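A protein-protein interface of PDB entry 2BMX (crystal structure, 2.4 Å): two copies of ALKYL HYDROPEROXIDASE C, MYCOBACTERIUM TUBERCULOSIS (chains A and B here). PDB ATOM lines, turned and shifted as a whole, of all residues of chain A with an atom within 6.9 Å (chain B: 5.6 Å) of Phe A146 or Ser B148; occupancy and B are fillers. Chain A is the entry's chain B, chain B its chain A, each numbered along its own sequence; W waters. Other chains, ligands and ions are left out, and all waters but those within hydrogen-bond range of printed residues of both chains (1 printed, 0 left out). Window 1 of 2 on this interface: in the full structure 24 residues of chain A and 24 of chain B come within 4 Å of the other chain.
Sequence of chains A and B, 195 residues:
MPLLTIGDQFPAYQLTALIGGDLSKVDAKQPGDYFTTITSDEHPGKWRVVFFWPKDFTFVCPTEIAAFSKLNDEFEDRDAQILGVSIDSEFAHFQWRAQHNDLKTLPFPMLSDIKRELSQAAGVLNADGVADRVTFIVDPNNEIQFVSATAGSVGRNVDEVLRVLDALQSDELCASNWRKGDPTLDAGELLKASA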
ATOM      1  N   LEU A   4      29.113  11.762 -11.549  1.00  0.00           N
ATOM      2  CA  LEU A   4      29.447  12.783 -10.587  1.00  0.00           C
ATOM      3  C   LEU A   4      28.580  12.538  -9.330  1.00  0.00           C
ATOM      4  O   LEU A   4      27.438  12.042  -9.414  1.00  0.00           O
ATOM      5  CB  LEU A   4      29.195  14.164 -11.187  1.00  0.00           C
ATOM      6  CG  LEU A   4      30.274  15.112 -11.795  1.00  0.00           C
ATOM      7  CD1 LEU A   4      31.703  14.594 -12.197  1.00  0.00           C
ATOM      8  CD2 LEU A   4      29.692  16.045 -12.819  1.00  0.00           C
ATOM      9  N   THR A   5      29.128  12.877  -8.159  1.00  0.00           N
ATOM     10  CA  THR A   5      28.479  12.549  -6.902  1.00  0.00           C
ATOM     11  C   THR A   5      28.358  13.745  -5.942  1.00  0.00           C
ATOM     12  O   THR A   5      28.696  14.882  -6.297  1.00  0.00           O
ATOM     13  CB  THR A   5      29.159  11.293  -6.225  1.00  0.00           C
ATOM     14  OG1 THR A   5      28.393  10.900  -5.083  1.00  0.00           O
ATOM     15  CG2 THR A   5      30.643  11.572  -5.817  1.00  0.00           C
ATOM     16  N   ILE A   6      27.838  13.462  -4.745  1.00  0.00           N
ATOM     17  CA  ILE A   6      27.634  14.420  -3.675  1.00  0.00           C
ATOM     18  C   ILE A   6      28.914  15.265  -3.488  1.00  0.00           C
ATOM     19  O   ILE A   6      30.011  14.712  -3.294  1.00  0.00           O
ATOM     20  CB  ILE A   6      27.280  13.682  -2.320  1.00  0.00           C
ATOM     21  CG1 ILE A   6      26.102  12.698  -2.506  1.00  0.00           C
ATOM     22  CG2 ILE A   6      27.026  14.687  -1.151  1.00  0.00           C
ATOM     23  CD1 ILE A   6      24.822  13.341  -3.068  1.00  0.00           C
ATOM     24  N   GLY A   7      28.767  16.586  -3.505  1.00  0.00           N
ATOM     25  CA  GLY A   7      29.926  17.457  -3.301  1.00  0.00           C
ATOM     26  C   GLY A   7      30.610  17.880  -4.600  1.00  0.00           C
ATOM     27  O   GLY A   7      31.401  18.793  -4.593  1.00  0.00           O
ATOM     28  N   VAL A  49      17.027  21.003 -10.576  1.00  0.00           N
ATOM     29  CA  VAL A  49      16.674  19.574 -10.559  1.00  0.00           C
ATOM     30  C   VAL A  49      16.762  19.078 -12.007  1.00  0.00           C
ATOM     31  O   VAL A  49      15.901  19.403 -12.844  1.00  0.00           O
ATOM     32  CB  VAL A  49      15.283  19.309  -9.912  1.00  0.00           C
ATOM     33  CG1 VAL A  49      15.007  17.793  -9.750  1.00  0.00           C
ATOM     34  CG2 VAL A  49      15.186  20.008  -8.546  1.00  0.00           C
ATOM     35  N   THR A 135      18.827  11.498 -12.133  1.00  0.00           N
ATOM     36  CA  THR A 135      18.384  12.762 -11.539  1.00  0.00           C
ATOM     37  C   THR A 135      19.503  13.358 -10.683  1.00  0.00           C
ATOM     38  O   THR A 135      20.108  12.671  -9.864  1.00  0.00           O
ATOM     39  CB  THR A 135      17.102  12.531 -10.653  1.00  0.00           C
ATOM     40  OG1 THR A 135      16.141  11.780 -11.401  1.00  0.00           O
ATOM     41  CG2 THR A 135      16.468  13.813 -10.267  1.00  0.00           C
ATOM     42  N   PHE A 136      19.728  14.641 -10.837  1.00  0.00           N
ATOM     43  CA  PHE A 136      20.594  15.401  -9.949  1.00  0.00           C
ATOM     44  C   PHE A 136      19.817  16.487  -9.261  1.00  0.00           C
ATOM     45  O   PHE A 136      18.959  17.129  -9.878  1.00  0.00           O
ATOM     46  CB  PHE A 136      21.710  16.104 -10.726  1.00  0.00           C
ATOM     47  CG  PHE A 136      22.677  15.165 -11.346  1.00  0.00           C
ATOM     48  CD1 PHE A 136      22.450  14.646 -12.626  1.00  0.00           C
ATOM     49  CD2 PHE A 136      23.808  14.745 -10.638  1.00  0.00           C
ATOM     50  CE1 PHE A 136      23.374  13.728 -13.210  1.00  0.00           C
ATOM     51  CE2 PHE A 136      24.749  13.855 -11.238  1.00  0.00           C
ATOM     52  CZ  PHE A 136      24.537  13.362 -12.514  1.00  0.00           C
ATOM     53  N   ILE A 137      20.147  16.716  -7.982  1.00  0.00           N
ATOM     54  CA  ILE A 137      19.776  17.961  -7.339  1.00  0.00           C
ATOM     55  C   ILE A 137      21.082  18.731  -7.126  1.00  0.00           C
ATOM     56  O   ILE A 137      22.017  18.218  -6.507  1.00  0.00           O
ATOM     57  CB  ILE A 137      19.023  17.753  -6.015  1.00  0.00           C
ATOM     58  CG1 ILE A 137      17.653  17.100  -6.273  1.00  0.00           C
ATOM     59  CG2 ILE A 137      18.843  19.065  -5.317  1.00  0.00           C
ATOM     60  CD1 ILE A 137      16.945  16.717  -5.023  1.00  0.00           C
ATOM     61  N   VAL A 138      21.127  19.946  -7.671  1.00  0.00           N
ATOM     62  CA  VAL A 138      22.248  20.815  -7.524  1.00  0.00           C
ATOM     63  C   VAL A 138      21.900  22.126  -6.871  1.00  0.00           C
ATOM     64  O   VAL A 138      20.886  22.775  -7.221  1.00  0.00           O
ATOM     65  CB  VAL A 138      23.179  20.928  -8.852  1.00  0.00           C
ATOM     66  CG1 VAL A 138      22.620  20.210 -10.102  1.00  0.00           C
ATOM     67  CG2 VAL A 138      23.686  22.313  -9.107  1.00  0.00           C
ATOM     68  N   GLU A 143      26.716  22.782  -6.545  1.00  0.00           N
ATOM     69  CA  GLU A 143      27.231  21.575  -5.917  1.00  0.00           C
ATOM     70  C   GLU A 143      26.189  20.471  -5.918  1.00  0.00           C
ATOM     71  O   GLU A 143      25.029  20.740  -5.666  1.00  0.00           O
ATOM     72  CB  GLU A 143      27.724  21.885  -4.484  1.00  0.00           C
ATOM     73  CG  GLU A 143      28.381  20.719  -3.802  1.00  0.00           C
ATOM     74  CD  GLU A 143      29.066  21.139  -2.478  1.00  0.00           C
ATOM     75  OE1 GLU A 143      30.105  21.848  -2.516  1.00  0.00           O
ATOM     76  OE2 GLU A 143      28.541  20.778  -1.408  1.00  0.00           O
ATOM     77  N   ILE A 144      26.592  19.230  -6.200  1.00  0.00           N
ATOM     78  CA  ILE A 144      25.625  18.139  -6.275  1.00  0.00           C
ATOM     79  C   ILE A 144      25.318  17.711  -4.858  1.00  0.00           C
ATOM     80  O   ILE A 144      26.269  17.504  -4.045  1.00  0.00           O
ATOM     81  CB  ILE A 144      26.138  16.969  -7.153  1.00  0.00           C
ATOM     82  CG1 ILE A 144      26.283  17.428  -8.617  1.00  0.00           C
ATOM     83  CG2 ILE A 144      25.226  15.675  -6.994  1.00  0.00           C
ATOM     84  CD1 ILE A 144      27.252  16.586  -9.445  1.00  0.00           C
ATOM     85  N   GLN A 145      24.009  17.689  -4.548  1.00  0.00           N
ATOM     86  CA  GLN A 145      23.486  17.243  -3.248  1.00  0.00           C
ATOM     87  C   GLN A 145      22.646  15.978  -3.356  1.00  0.00           C
ATOM     88  O   GLN A 145      22.236  15.404  -2.336  1.00  0.00           O
ATOM     89  CB  GLN A 145      22.650  18.351  -2.562  1.00  0.00           C
ATOM     90  CG  GLN A 145      23.367  19.724  -2.344  1.00  0.00           C
ATOM     91  CD  GLN A 145      24.645  19.619  -1.512  1.00  0.00           C
ATOM     92  OE1 GLN A 145      24.883  18.621  -0.819  1.00  0.00           O
ATOM     93  NE2 GLN A 145      25.478  20.654  -1.580  1.00  0.00           N
ATOM     94  N   PHE A 146      22.362  15.534  -4.588  1.00  0.00           N
ATOM     95  CA  PHE A 146      21.608  14.299  -4.785  1.00  0.00           C
ATOM     96  C   PHE A 146      21.837  13.824  -6.191  1.00  0.00           C
ATOM     97  O   PHE A 146      21.816  14.624  -7.115  1.00  0.00           O
ATOM     98  CB  PHE A 146      20.108  14.537  -4.531  1.00  0.00           C
ATOM     99  CG  PHE A 146      19.194  13.373  -4.941  1.00  0.00           C
ATOM    100  CD1 PHE A 146      19.069  12.263  -4.142  1.00  0.00           C
ATOM    101  CD2 PHE A 146      18.432  13.435  -6.108  1.00  0.00           C
ATOM    102  CE1 PHE A 146      18.218  11.199  -4.475  1.00  0.00           C
ATOM    103  CE2 PHE A 146      17.586  12.387  -6.459  1.00  0.00           C
ATOM    104  CZ  PHE A 146      17.473  11.276  -5.626  1.00  0.00           C
ATOM    105  N   VAL A 147      22.088  12.523  -6.333  1.00  0.00           N
ATOM    106  CA  VAL A 147      22.138  11.888  -7.618  1.00  0.00           C
ATOM    107  C   VAL A 147      21.473  10.507  -7.509  1.00  0.00           C
ATOM    108  O   VAL A 147      21.729   9.737  -6.563  1.00  0.00           O
ATOM    109  CB  VAL A 147      23.596  11.822  -8.221  1.00  0.00           C
ATOM    110  CG1 VAL A 147      24.567  11.114  -7.302  1.00  0.00           C
ATOM    111  CG2 VAL A 147      23.581  11.187  -9.617  1.00  0.00           C
ATOM    112  N   SER A 148      20.620  10.188  -8.484  1.00  0.00           N
ATOM    113  CA  SER A 148      19.950   8.902  -8.493  1.00  0.00           C
ATOM    114  C   SER A 148      19.945   8.338  -9.898  1.00  0.00           C
ATOM    115  O   SER A 148      19.639   9.063 -10.836  1.00  0.00           O
ATOM    116  CB  SER A 148      18.532   9.058  -7.979  1.00  0.00           C
ATOM    117  OG  SER A 148      18.052   7.785  -7.674  1.00  0.00           O
ATOM    118  N   ALA A 149      20.277   7.044 -10.062  1.00  0.00           N
ATOM    119  CA  ALA A 149      20.349   6.465 -11.407  1.00  0.00           C
ATOM    120  C   ALA A 149      19.670   5.142 -11.417  1.00  0.00           C
ATOM    121  O   ALA A 149      19.763   4.415 -10.460  1.00  0.00           O
ATOM    122  CB  ALA A 149      21.803   6.332 -11.884  1.00  0.00           C
ATOM    123  N   GLU A 160       9.337  11.580  -4.556  1.00  0.00           N
ATOM    124  CA  GLU A 160      10.568  11.291  -3.844  1.00  0.00           C
ATOM    125  C   GLU A 160      11.683  12.354  -4.030  1.00  0.00           C
ATOM    126  O   GLU A 160      12.315  12.768  -3.059  1.00  0.00           O
ATOM    127  CB  GLU A 160      11.028   9.875  -4.210  1.00  0.00           C
ATOM    128  CG  GLU A 160      12.337   9.456  -3.563  1.00  0.00           C
ATOM    129  CD  GLU A 160      12.287   9.369  -2.024  1.00  0.00           C
ATOM    130  OE1 GLU A 160      11.204   9.365  -1.391  1.00  0.00           O
ATOM    131  OE2 GLU A 160      13.382   9.286  -1.444  1.00  0.00           O
ATOM    132  N   VAL A 161      11.896  12.800  -5.261  1.00  0.00           N
ATOM    133  CA  VAL A 161      12.864  13.859  -5.595  1.00  0.00           C
ATOM    134  C   VAL A 161      12.495  15.177  -4.906  1.00  0.00           C
ATOM    135  O   VAL A 161      13.319  15.860  -4.332  1.00  0.00           O
ATOM    136  CB  VAL A 161      12.929  14.061  -7.152  1.00  0.00           C
ATOM    137  CG1 VAL A 161      13.905  15.231  -7.564  1.00  0.00           C
ATOM    138  CG2 VAL A 161      13.309  12.757  -7.828  1.00  0.00           C
ATOM    139  N   VAL A 164      13.363  14.777  -1.138  1.00  0.00           N
ATOM    140  CA  VAL A 164      14.787  14.944  -0.928  1.00  0.00           C
ATOM    141  C   VAL A 164      15.140  16.427  -0.999  1.00  0.00           C
ATOM    142  O   VAL A 164      15.868  16.931  -0.146  1.00  0.00           O
ATOM    143  CB  VAL A 164      15.572  14.141  -1.986  1.00  0.00           C
ATOM    144  CG1 VAL A 164      17.032  14.422  -1.878  1.00  0.00           C
ATOM    145  CG2 VAL A 164      15.276  12.662  -1.823  1.00  0.00           C
ATOM    146  N   LEU A 165      14.632  17.116  -2.010  1.00  0.00           N
ATOM    147  CA  LEU A 165      14.855  18.554  -2.160  1.00  0.00           C
ATOM    148  C   LEU A 165      14.395  19.269  -0.906  1.00  0.00           C
ATOM    149  O   LEU A 165      15.131  20.066  -0.324  1.00  0.00           O
ATOM    150  CB  LEU A 165      14.121  19.140  -3.381  1.00  0.00           C
ATOM    151  CG  LEU A 165      14.229  20.679  -3.544  1.00  0.00           C
ATOM    152  CD1 LEU A 165      15.699  21.177  -3.727  1.00  0.00           C
ATOM    153  CD2 LEU A 165      13.282  21.247  -4.625  1.00  0.00           C
ATOM    154  N   LEU A 168      16.693  18.461   2.010  1.00  0.00           N
ATOM    155  CA  LEU A 168      17.982  19.136   1.905  1.00  0.00           C
ATOM    156  C   LEU A 168      17.926  20.589   2.356  1.00  0.00           C
ATOM    157  O   LEU A 168      18.919  21.113   2.855  1.00  0.00           O
ATOM    158  CB  LEU A 168      18.564  19.079   0.490  1.00  0.00           C
ATOM    159  CG  LEU A 168      19.070  17.716   0.037  1.00  0.00           C
ATOM    160  CD1 LEU A 168      19.149  17.696  -1.481  1.00  0.00           C
ATOM    161  CD2 LEU A 168      20.405  17.390   0.721  1.00  0.00           C
ATOM    162  N   ARG B 133      25.851   8.632   2.292  1.00  0.00           N
ATOM    163  CA  ARG B 133      24.594   7.881   2.314  1.00  0.00           C
ATOM    164  C   ARG B 133      24.180   7.430   0.913  1.00  0.00           C
ATOM    165  O   ARG B 133      23.561   8.193   0.170  1.00  0.00           O
ATOM    166  CB  ARG B 133      23.478   8.768   2.817  1.00  0.00           C
ATOM    167  CG  ARG B 133      23.321   8.757   4.230  1.00  0.00           C
ATOM    168  CD  ARG B 133      21.856   8.571   4.672  1.00  0.00           C
ATOM    169  NE  ARG B 133      21.944   8.527   6.127  1.00  0.00           N
ATOM    170  CZ  ARG B 133      22.449   9.533   6.829  1.00  0.00           C
ATOM    171  NH1 ARG B 133      22.827  10.624   6.181  1.00  0.00           N
ATOM    172  NH2 ARG B 133      22.552   9.465   8.153  1.00  0.00           N
ATOM    173  N   VAL B 134      24.508   6.196   0.561  1.00  0.00           N
ATOM    174  CA  VAL B 134      24.361   5.726  -0.791  1.00  0.00           C
ATOM    175  C   VAL B 134      23.720   4.340  -0.735  1.00  0.00           C
ATOM    176  O   VAL B 134      24.157   3.522   0.074  1.00  0.00           O
ATOM    177  CB  VAL B 134      25.748   5.590  -1.500  1.00  0.00           C
ATOM    178  CG1 VAL B 134      25.574   5.158  -2.929  1.00  0.00           C
ATOM    179  CG2 VAL B 134      26.562   6.867  -1.422  1.00  0.00           C
ATOM    180  N   THR B 135      22.697   4.106  -1.586  1.00  0.00           N
ATOM    181  CA  THR B 135      22.103   2.805  -1.802  1.00  0.00           C
ATOM    182  C   THR B 135      22.462   2.334  -3.207  1.00  0.00           C
ATOM    183  O   THR B 135      22.349   3.113  -4.171  1.00  0.00           O
ATOM    184  CB  THR B 135      20.536   2.845  -1.750  1.00  0.00           C
ATOM    185  OG1 THR B 135      20.107   3.581  -0.599  1.00  0.00           O
ATOM    186  CG2 THR B 135      19.932   1.411  -1.703  1.00  0.00           C
ATOM    187  N   PHE B 136      22.825   1.052  -3.303  1.00  0.00           N
ATOM    188  CA  PHE B 136      23.044   0.370  -4.558  1.00  0.00           C
ATOM    189  C   PHE B 136      22.128  -0.857  -4.682  1.00  0.00           C
ATOM    190  O   PHE B 136      21.920  -1.586  -3.709  1.00  0.00           O
ATOM    191  CB  PHE B 136      24.484  -0.189  -4.667  1.00  0.00           C
ATOM    192  CG  PHE B 136      25.563   0.861  -4.752  1.00  0.00           C
ATOM    193  CD1 PHE B 136      26.210   1.302  -3.585  1.00  0.00           C
ATOM    194  CD2 PHE B 136      26.009   1.327  -6.003  1.00  0.00           C
ATOM    195  CE1 PHE B 136      27.243   2.287  -3.668  1.00  0.00           C
ATOM    196  CE2 PHE B 136      27.055   2.317  -6.114  1.00  0.00           C
ATOM    197  CZ  PHE B 136      27.658   2.794  -4.949  1.00  0.00           C
ATOM    198  N   PHE B 146      20.960   0.187  -9.856  1.00  0.00           N
ATOM    199  CA  PHE B 146      20.446   1.351  -9.191  1.00  0.00           C
ATOM    200  C   PHE B 146      21.495   1.902  -8.230  1.00  0.00           C
ATOM    201  O   PHE B 146      22.154   1.120  -7.536  1.00  0.00           O
ATOM    202  CB  PHE B 146      19.129   1.007  -8.471  1.00  0.00           C
ATOM    203  CG  PHE B 146      18.608   2.112  -7.541  1.00  0.00           C
ATOM    204  CD1 PHE B 146      17.939   3.233  -8.051  1.00  0.00           C
ATOM    205  CD2 PHE B 146      18.756   1.996  -6.153  1.00  0.00           C
ATOM    206  CE1 PHE B 146      17.426   4.197  -7.205  1.00  0.00           C
ATOM    207  CE2 PHE B 146      18.251   2.975  -5.302  1.00  0.00           C
ATOM    208  CZ  PHE B 146      17.580   4.056  -5.812  1.00  0.00           C
ATOM    209  N   VAL B 147      21.668   3.239  -8.208  1.00  0.00           N
ATOM    210  CA  VAL B 147      22.496   3.867  -7.221  1.00  0.00           C
ATOM    211  C   VAL B 147      21.751   5.125  -6.853  1.00  0.00           C
ATOM    212  O   VAL B 147      21.266   5.832  -7.723  1.00  0.00           O
ATOM    213  CB  VAL B 147      23.850   4.512  -7.739  1.00  0.00           C
ATOM    214  CG1 VAL B 147      24.961   4.553  -6.595  1.00  0.00           C
ATOM    215  CG2 VAL B 147      24.313   4.086  -9.097  1.00  0.00           C
ATOM    216  N   SER B 148      21.804   5.485  -5.587  1.00  0.00           N
ATOM    217  CA  SER B 148      21.185   6.708  -5.056  1.00  0.00           C
ATOM    218  C   SER B 148      22.078   7.254  -3.989  1.00  0.00           C
ATOM    219  O   SER B 148      22.457   6.515  -3.091  1.00  0.00           O
ATOM    220  CB  SER B 148      19.853   6.409  -4.395  1.00  0.00           C
ATOM    221  OG  SER B 148      19.047   7.562  -4.466  1.00  0.00           O
ATOM    222  N   ALA B 149      22.402   8.535  -4.074  1.00  0.00           N
ATOM    223  CA  ALA B 149      23.341   9.153  -3.154  1.00  0.00           C
ATOM    224  C   ALA B 149      22.723  10.433  -2.694  1.00  0.00           C
ATOM    225  O   ALA B 149      22.124  11.138  -3.486  1.00  0.00           O
ATOM    226  CB  ALA B 149      24.688   9.416  -3.841  1.00  0.00           C
ATOM    227  N   THR B 150      22.863  10.730  -1.413  1.00  0.00           N
ATOM    228  CA  THR B 150      22.236  11.886  -0.824  1.00  0.00           C
ATOM    229  C   THR B 150      23.223  12.612   0.118  1.00  0.00           C
ATOM    230  O   THR B 150      24.055  11.978   0.789  1.00  0.00           O
ATOM    231  CB  THR B 150      20.922  11.461  -0.104  1.00  0.00           C
ATOM    232  OG1 THR B 150      19.999  12.500  -0.204  1.00  0.00           O
ATOM    233  CG2 THR B 150      21.121  11.221   1.364  1.00  0.00           C
ATOM    234  N   ALA B 151      23.152  13.933   0.160  1.00  0.00           N
ATOM    235  CA  ALA B 151      23.995  14.640   1.080  1.00  0.00           C
ATOM    236  C   ALA B 151      23.367  14.628   2.489  1.00  0.00           C
ATOM    237  O   ALA B 151      22.199  14.268   2.664  1.00  0.00           O
ATOM    238  CB  ALA B 151      24.196  16.082   0.613  1.00  0.00           C
HETATM  239  O   HOH W   1      16.118   7.701  -4.991  1.00  0.00           O
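N of Ala B149 lies within hydrogen-bond range of O of Val A147, at 2.8 Å.
The backbone NH of Ala B151 lies within hydrogen-bond range of the backbone carbonyl oxygen of Gln A145 (3.0 Å).
The side-chain hydroxyl (OG) of Ser B148 is in hydrogen-bond range of the side-chain hydroxyl (OG) of Ser A148 (3.4 Å).
The backbone NH of Ala A149 lies within hydrogen-bond range of the backbone carbonyl oxygen of Val B147 (2.8 Å).
N of Thr A135 lies within hydrogen-bond range of O of Ser A148 (2.9 Å).
OE2 of Glu A143 sits at hydrogen-bond distance from NE2 of Gln A145.
The backbone NH (N) of Ser B148 sits at hydrogen-bond distance from the backbone carbonyl oxygen (O) of Thr B135, at 2.8 Å.
O of Phe A146 lies within hydrogen-bond range of N of Ile A137 (2.8 Å).
N of Thr B150 lies within hydrogen-bond range of O of Arg B133, 3.1 Å away.
The backbone carbonyl oxygen (O) of Ile A137 lies within hydrogen-bond range of the backbone NH (N) of Gln A145 (2.8 Å).
Among the printed residues, pairs that only touch across the chains: Ile A6 with Ala B149 (3.5 Å), Ile A6 with Thr B150 (3.6 Å), Ile A6 with Ala B151 (3.6 Å), Gln A145 with Thr B150 (3.8 Å), Phe A146 with Ser B148 (3.7 Å), Phe A146 with Ala B149 (3.3 Å), Val A147 with Ser B148 (3.4 Å), Ser A148 with Phe B146 (3.7 Å), Ser A148 with Val B147 (3.4 Å), Ala A149 with Phe B146 (3.2 Å) and Val A164 with Thr B150 (3.9 Å).
Gly A7 touches none of the printed residues of chain B.
Val A138 touches none of the printed residues of chain B.
Printed residues of chain B within 4 Å of Gln A145: Thr B150 and Ala B151.
Printed residues of chain B within 4 Å of Phe A146: Ser B148 and Ala B149.
Printed residues of chain B within 4 Å of Val A147: Ser B148 (3.4 Å) and Ala B149 (2.8 Å).
Of the printed residues of chain B, Ala A149 touches Phe B146 and Val B147.
Ser B148 touches just these residues of chain A: Phe A146 (3.7 Å), Val A147 (3.4 Å) and Ser A148 (3.4 Å).
Of the printed residues of chain A, Ala B149 touches Ile A6 (3.5 Å), Phe A146 (3.3 Å) and Val A147 (2.8 Å).
The nearest residue of chain B that does not touch Phe A146 is Thr B150 (4.1 Å).
The nearest printed residue of chain B that does not touch Gln A145 is Ala B149 (4.4 Å).
Of the 10 printed residues of chain B, 6 touch a printed residue of chain A.
Hydrophobic or aromatic side chains of chain B that line the printed part of chain A: Phe B146, Ala B149 and Ala B151.
Along chain B the printed residues that touch a printed residue of chain A span positions 146 to 151.
Of the 21 printed residues of chain A, 7 touch a printed residue of chain B.
Hydrophobic or aromatic side chains of chain A within 4 Å of the printed part of chain B: Ile A6, Phe A146, Val A147 and Val A164.
Phe A146 touches Ser B148, and with the chains exchanged Ser A148 touches Phe B146.
Phe A146 touches Ala B149, and with the chains exchanged Ala A149 touches Phe B146.
Val A147 touches Ser B148, and with the chains exchanged Ser A148 touches Val B147.
Val A147 touches Ala B149, and with the chains exchanged Ala A149 touches Val B147.
Of the 15 pairs that touch across the chains among the printed residues, 9 have their exchanged pair printed and touching as well.
Water W1 lies within hydrogen-bond range of the side-chain hydroxyl (OG) of Ser B148 and the side-chain hydroxyl (OG) of Ser A148.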
